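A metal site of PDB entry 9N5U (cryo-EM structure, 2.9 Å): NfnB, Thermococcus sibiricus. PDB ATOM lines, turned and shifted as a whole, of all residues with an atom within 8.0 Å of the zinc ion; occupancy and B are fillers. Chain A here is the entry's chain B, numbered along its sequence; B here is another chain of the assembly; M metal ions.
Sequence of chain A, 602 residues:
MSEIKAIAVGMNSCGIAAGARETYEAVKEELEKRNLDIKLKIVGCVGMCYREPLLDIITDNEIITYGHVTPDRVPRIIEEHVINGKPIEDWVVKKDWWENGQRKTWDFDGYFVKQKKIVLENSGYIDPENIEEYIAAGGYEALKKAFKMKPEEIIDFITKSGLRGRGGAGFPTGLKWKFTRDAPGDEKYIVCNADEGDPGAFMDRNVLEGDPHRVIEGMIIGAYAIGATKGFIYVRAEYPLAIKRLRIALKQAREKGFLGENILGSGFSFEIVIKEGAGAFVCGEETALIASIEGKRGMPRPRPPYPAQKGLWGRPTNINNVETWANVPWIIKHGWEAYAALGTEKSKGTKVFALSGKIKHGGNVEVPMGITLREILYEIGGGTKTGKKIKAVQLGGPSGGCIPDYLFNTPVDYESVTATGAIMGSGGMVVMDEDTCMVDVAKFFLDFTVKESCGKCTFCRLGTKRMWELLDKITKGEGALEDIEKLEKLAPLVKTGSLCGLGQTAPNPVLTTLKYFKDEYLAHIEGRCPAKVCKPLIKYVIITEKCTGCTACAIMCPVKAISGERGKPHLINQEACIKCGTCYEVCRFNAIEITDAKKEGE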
ATOM      1  N   GLY A  10       8.579   2.893 -34.956  1.00  0.00           N
ATOM      2  CA  GLY A  10       8.337   3.228 -33.564  1.00  0.00           C
ATOM      3  C   GLY A  10       9.037   4.504 -33.164  1.00  0.00           C
ATOM      4  O   GLY A  10      10.271   4.599 -33.246  1.00  0.00           O
ATOM      5  N   ASN A  12       8.752   6.475 -30.085  1.00  0.00           N
ATOM      6  CA  ASN A  12       8.729   6.892 -28.692  1.00  0.00           C
ATOM      7  C   ASN A  12      10.101   7.427 -28.304  1.00  0.00           C
ATOM      8  O   ASN A  12      11.030   7.470 -29.109  1.00  0.00           O
ATOM      9  CB  ASN A  12       8.307   5.730 -27.784  1.00  0.00           C
ATOM     10  CG  ASN A  12       6.899   5.877 -27.276  1.00  0.00           C
ATOM     11  OD1 ASN A  12       6.071   6.557 -27.873  1.00  0.00           O
ATOM     12  ND2 ASN A  12       6.617   5.243 -26.144  1.00  0.00           N
ATOM     13  N   SER A  13      10.244   7.839 -27.038  1.00  0.00           N
ATOM     14  CA  SER A  13      11.533   8.322 -26.561  1.00  0.00           C
ATOM     15  C   SER A  13      12.595   7.233 -26.629  1.00  0.00           C
ATOM     16  O   SER A  13      13.753   7.494 -26.994  1.00  0.00           O
ATOM     17  CB  SER A  13      11.399   8.866 -25.144  1.00  0.00           C
ATOM     18  OG  SER A  13      10.447   9.907 -25.096  1.00  0.00           O
ATOM     19  N   CYS A  14      12.217   6.005 -26.277  1.00  0.00           N
ATOM     20  CA  CYS A  14      13.134   4.873 -26.387  1.00  0.00           C
ATOM     21  C   CYS A  14      13.529   4.623 -27.838  1.00  0.00           C
ATOM     22  O   CYS A  14      14.693   4.314 -28.131  1.00  0.00           O
ATOM     23  CB  CYS A  14      12.502   3.631 -25.780  1.00  0.00           C
ATOM     24  SG  CYS A  14      10.849   3.280 -26.383  1.00  0.00           S
ATOM     25  N   GLY A  15      12.568   4.709 -28.760  1.00  0.00           N
ATOM     26  CA  GLY A  15      12.893   4.553 -30.160  1.00  0.00           C
ATOM     27  C   GLY A  15      13.739   5.696 -30.689  1.00  0.00           C
ATOM     28  O   GLY A  15      14.688   5.475 -31.448  1.00  0.00           O
ATOM     29  N   ILE A  16      13.415   6.922 -30.297  1.00  0.00           N
ATOM     30  CA  ILE A  16      14.149   8.095 -30.758  1.00  0.00           C
ATOM     31  C   ILE A  16      15.606   8.023 -30.305  1.00  0.00           C
ATOM     32  O   ILE A  16      16.522   8.370 -31.065  1.00  0.00           O
ATOM     33  CB  ILE A  16      13.458   9.381 -30.265  1.00  0.00           C
ATOM     34  CG1 ILE A  16      12.182   9.635 -31.055  1.00  0.00           C
ATOM     35  CG2 ILE A  16      14.387  10.576 -30.376  1.00  0.00           C
ATOM     36  CD1 ILE A  16      11.375  10.791 -30.543  1.00  0.00           C
ATOM     37  N   GLY A  44       3.938   4.070 -31.455  1.00  0.00           N
ATOM     38  CA  GLY A  44       4.580   4.143 -30.153  1.00  0.00           C
ATOM     39  C   GLY A  44       5.550   3.003 -29.912  1.00  0.00           C
ATOM     40  O   GLY A  44       6.297   2.618 -30.810  1.00  0.00           O
ATOM     41  N   CYS A  45       5.539   2.465 -28.702  1.00  0.00           N
ATOM     42  CA  CYS A  45       6.398   1.352 -28.329  1.00  0.00           C
ATOM     43  C   CYS A  45       5.532   0.142 -28.009  1.00  0.00           C
ATOM     44  O   CYS A  45       4.669   0.217 -27.135  1.00  0.00           O
ATOM     45  CB  CYS A  45       7.276   1.717 -27.133  1.00  0.00           C
ATOM     46  SG  CYS A  45       8.314   0.383 -26.527  1.00  0.00           S
ATOM     47  N   VAL A  46       5.767  -0.966 -28.705  1.00  0.00           N
ATOM     48  CA  VAL A  46       5.064  -2.196 -28.365  1.00  0.00           C
ATOM     49  C   VAL A  46       5.549  -2.726 -27.026  1.00  0.00           C
ATOM     50  O   VAL A  46       4.767  -3.187 -26.193  1.00  0.00           O
ATOM     51  CB  VAL A  46       5.195  -3.243 -29.481  1.00  0.00           C
ATOM     52  CG1 VAL A  46       4.268  -2.912 -30.627  1.00  0.00           C
ATOM     53  CG2 VAL A  46       6.619  -3.326 -29.966  1.00  0.00           C
ATOM     54  N   GLY A  47       6.855  -2.647 -26.777  1.00  0.00           N
ATOM     55  CA  GLY A  47       7.418  -3.129 -25.534  1.00  0.00           C
ATOM     56  C   GLY A  47       8.787  -3.747 -25.698  1.00  0.00           C
ATOM     57  O   GLY A  47       9.537  -3.861 -24.719  1.00  0.00           O
ATOM     58  N   MET A  48       9.144  -4.140 -26.918  1.00  0.00           N
ATOM     59  CA  MET A  48      10.449  -4.739 -27.190  1.00  0.00           C
ATOM     60  C   MET A  48      11.487  -3.630 -27.355  1.00  0.00           C
ATOM     61  O   MET A  48      11.995  -3.347 -28.440  1.00  0.00           O
ATOM     62  CB  MET A  48      10.393  -5.621 -28.432  1.00  0.00           C
ATOM     63  CG  MET A  48       9.221  -6.564 -28.489  1.00  0.00           C
ATOM     64  SD  MET A  48       9.296  -7.690 -29.889  1.00  0.00           S
ATOM     65  CE  MET A  48      10.320  -8.988 -29.215  1.00  0.00           C
ATOM     66  N   CYS A  49      11.805  -2.990 -26.229  1.00  0.00           N
ATOM     67  CA  CYS A  49      12.789  -1.914 -26.230  1.00  0.00           C
ATOM     68  C   CYS A  49      14.202  -2.433 -26.493  1.00  0.00           C
ATOM     69  O   CYS A  49      15.071  -1.651 -26.895  1.00  0.00           O
ATOM     70  CB  CYS A  49      12.758  -1.168 -24.897  1.00  0.00           C
ATOM     71  SG  CYS A  49      11.199  -0.331 -24.538  1.00  0.00           S
ATOM     72  N   TYR A  50      14.438  -3.727 -26.292  1.00  0.00           N
ATOM     73  CA  TYR A  50      15.752  -4.291 -26.573  1.00  0.00           C
ATOM     74  C   TYR A  50      15.972  -4.572 -28.052  1.00  0.00           C
ATOM     75  O   TYR A  50      17.118  -4.714 -28.475  1.00  0.00           O
ATOM     76  CB  TYR A  50      15.956  -5.568 -25.750  1.00  0.00           C
ATOM     77  CG  TYR A  50      14.979  -6.681 -26.053  1.00  0.00           C
ATOM     78  CD1 TYR A  50      13.676  -6.640 -25.573  1.00  0.00           C
ATOM     79  CD2 TYR A  50      15.367  -7.786 -26.783  1.00  0.00           C
ATOM     80  CE1 TYR A  50      12.793  -7.662 -25.838  1.00  0.00           C
ATOM     81  CE2 TYR A  50      14.490  -8.803 -27.054  1.00  0.00           C
ATOM     82  CZ  TYR A  50      13.203  -8.747 -26.578  1.00  0.00           C
ATOM     83  OH  TYR A  50      12.330  -9.760 -26.841  1.00  0.00           O
ATOM     84  N   ARG A  51      14.904  -4.628 -28.841  1.00  0.00           N
ATOM     85  CA  ARG A  51      14.972  -4.951 -30.255  1.00  0.00           C
ATOM     86  C   ARG A  51      14.837  -3.729 -31.159  1.00  0.00           C
ATOM     87  O   ARG A  51      14.684  -3.888 -32.372  1.00  0.00           O
ATOM     88  CB  ARG A  51      13.867  -5.961 -30.602  1.00  0.00           C
ATOM     89  CG  ARG A  51      14.343  -7.172 -31.376  1.00  0.00           C
ATOM     90  CD  ARG A  51      15.153  -8.112 -30.520  1.00  0.00           C
ATOM     91  NE  ARG A  51      15.522  -9.314 -31.256  1.00  0.00           N
ATOM     92  CZ  ARG A  51      16.438 -10.180 -30.855  1.00  0.00           C
ATOM     93  NH1 ARG A  51      17.106 -10.005 -29.732  1.00  0.00           N
ATOM     94  NH2 ARG A  51      16.703 -11.245 -31.616  1.00  0.00           N
ATOM     95  N   GLU A  52      14.898  -2.527 -30.590  1.00  0.00           N
ATOM     96  CA  GLU A  52      14.664  -1.295 -31.335  1.00  0.00           C
ATOM     97  C   GLU A  52      15.893  -0.899 -32.150  1.00  0.00           C
ATOM     98  O   GLU A  52      17.026  -1.282 -31.819  1.00  0.00           O
ATOM     99  CB  GLU A  52      14.283  -0.189 -30.368  1.00  0.00           C
ATOM    100  CG  GLU A  52      12.917  -0.398 -29.745  1.00  0.00           C
ATOM    101  CD  GLU A  52      12.491   0.757 -28.875  1.00  0.00           C
ATOM    102  OE1 GLU A  52      13.380   1.504 -28.409  1.00  0.00           O
ATOM    103  OE2 GLU A  52      11.276   0.922 -28.660  1.00  0.00           O
ATOM    104  N   LEU A  54      12.282  -0.455 -34.307  1.00  0.00           N
ATOM    105  CA  LEU A  54      11.331  -1.424 -34.832  1.00  0.00           C
ATOM    106  C   LEU A  54      10.605  -0.835 -36.035  1.00  0.00           C
ATOM    107  O   LEU A  54      10.080   0.282 -35.961  1.00  0.00           O
ATOM    108  CB  LEU A  54      10.330  -1.841 -33.757  1.00  0.00           C
ATOM    109  CG  LEU A  54      10.845  -2.776 -32.667  1.00  0.00           C
ATOM    110  CD1 LEU A  54       9.778  -3.010 -31.623  1.00  0.00           C
ATOM    111  CD2 LEU A  54      11.301  -4.084 -33.269  1.00  0.00           C
ATOM    112  N   PHE A 202       9.761   4.321 -16.721  1.00  0.00           N
ATOM    113  CA  PHE A 202       9.462   4.980 -17.983  1.00  0.00           C
ATOM    114  C   PHE A 202       8.100   4.583 -18.518  1.00  0.00           C
ATOM    115  O   PHE A 202       7.791   4.894 -19.674  1.00  0.00           O
ATOM    116  CB  PHE A 202      10.544   4.670 -19.024  1.00  0.00           C
ATOM    117  CG  PHE A 202      10.971   3.226 -19.037  1.00  0.00           C
ATOM    118  CD1 PHE A 202      10.306   2.299 -19.813  1.00  0.00           C
ATOM    119  CD2 PHE A 202      12.051   2.792 -18.281  1.00  0.00           C
ATOM    120  CE1 PHE A 202      10.694   0.981 -19.835  1.00  0.00           C
ATOM    121  CE2 PHE A 202      12.444   1.477 -18.294  1.00  0.00           C
ATOM    122  CZ  PHE A 202      11.771   0.570 -19.075  1.00  0.00           C
ATOM    123  N   ASN A 206       5.657   6.292 -21.413  1.00  0.00           N
ATOM    124  CA  ASN A 206       5.345   5.363 -22.497  1.00  0.00           C
ATOM    125  C   ASN A 206       3.877   5.419 -22.860  1.00  0.00           C
ATOM    126  O   ASN A 206       3.516   5.435 -24.049  1.00  0.00           O
ATOM    127  CB  ASN A 206       5.752   3.948 -22.080  1.00  0.00           C
ATOM    128  CG  ASN A 206       5.848   2.994 -23.243  1.00  0.00           C
ATOM    129  OD1 ASN A 206       6.853   2.949 -23.941  1.00  0.00           O
ATOM    130  ND2 ASN A 206       4.800   2.209 -23.452  1.00  0.00           N
ATOM    131  N   GLY A 362      14.828  -6.417 -21.653  1.00  0.00           N
ATOM    132  CA  GLY A 362      14.314  -5.259 -20.945  1.00  0.00           C
ATOM    133  C   GLY A 362      13.346  -4.443 -21.797  1.00  0.00           C
ATOM    134  O   GLY A 362      13.499  -4.312 -23.007  1.00  0.00           O
ATOM    135  N   GLY A 363      12.349  -3.886 -21.128  1.00  0.00           N
ATOM    136  CA  GLY A 363      11.338  -3.107 -21.809  1.00  0.00           C
ATOM    137  C   GLY A 363      10.122  -2.929 -20.914  1.00  0.00           C
ATOM    138  O   GLY A 363      10.228  -2.983 -19.687  1.00  0.00           O
ATOM    139  N   ASN A 364       8.978  -2.717 -21.553  1.00  0.00           N
ATOM    140  CA  ASN A 364       7.717  -2.523 -20.866  1.00  0.00           C
ATOM    141  C   ASN A 364       6.886  -3.803 -20.967  1.00  0.00           C
ATOM    142  O   ASN A 364       6.553  -4.233 -22.068  1.00  0.00           O
ATOM    143  CB  ASN A 364       6.957  -1.335 -21.438  1.00  0.00           C
ATOM    144  CG  ASN A 364       7.660  -0.029 -21.206  1.00  0.00           C
ATOM    145  OD1 ASN A 364       8.444   0.421 -22.047  1.00  0.00           O
ATOM    146  ND2 ASN A 364       7.393   0.593 -20.072  1.00  0.00           N
ATOM    147  N   GLY B 117      14.642   7.312 -20.742  1.00  0.00           N
ATOM    148  CA  GLY B 117      13.740   6.395 -21.386  1.00  0.00           C
ATOM    149  C   GLY B 117      14.427   5.242 -22.091  1.00  0.00           C
ATOM    150  O   GLY B 117      13.787   4.203 -22.323  1.00  0.00           O
ATOM    151  N   CYS B 118      15.699   5.388 -22.436  1.00  0.00           N
ATOM    152  CA  CYS B 118      16.451   4.343 -23.130  1.00  0.00           C
ATOM    153  C   CYS B 118      17.298   3.544 -22.147  1.00  0.00           C
ATOM    154  O   CYS B 118      18.519   3.594 -22.149  1.00  0.00           O
ATOM    155  CB  CYS B 118      17.313   4.959 -24.224  1.00  0.00           C
ATOM    156  SG  CYS B 118      18.257   6.385 -23.691  1.00  0.00           S
ATOM    157  N   SER B 120      17.564   0.345 -22.154  1.00  0.00           N
ATOM    158  CA  SER B 120      18.227  -0.736 -22.866  1.00  0.00           C
ATOM    159  C   SER B 120      19.624  -0.354 -23.323  1.00  0.00           C
ATOM    160  O   SER B 120      20.532  -1.189 -23.262  1.00  0.00           O
ATOM    161  CB  SER B 120      17.402  -1.172 -24.074  1.00  0.00           C
ATOM    162  OG  SER B 120      18.016  -2.246 -24.745  1.00  0.00           O
HETATM  163 ZN    ZN M   1      10.499   1.021 -26.265  1.00  0.00          ZN
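The zinc ion is bound by SG of Cys 14 (2.3 Å), SG of Cys 45 (2.3 Å), SG of Cys 49 (2.3 Å) and OE2 of Glu 52 (2.5 Å).
The zinc ion has four donor atoms within binding distance.
Within 4 Å of the zinc ion: Cys 14, Cys 45, Cys 49 and Glu 52.
The side-chain sulfur (SG) of Cys 49 lies close to the side-chain amide oxygen (OD1) of Asn 364, 3.8 Å away.
SG of Cys 45 lies close to N of Gly 47 (3.4 Å).
The backbone NH of Gly 15 is in hydrogen-bond range of the side-chain carboxylate of Glu 52, 3.3 Å away.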
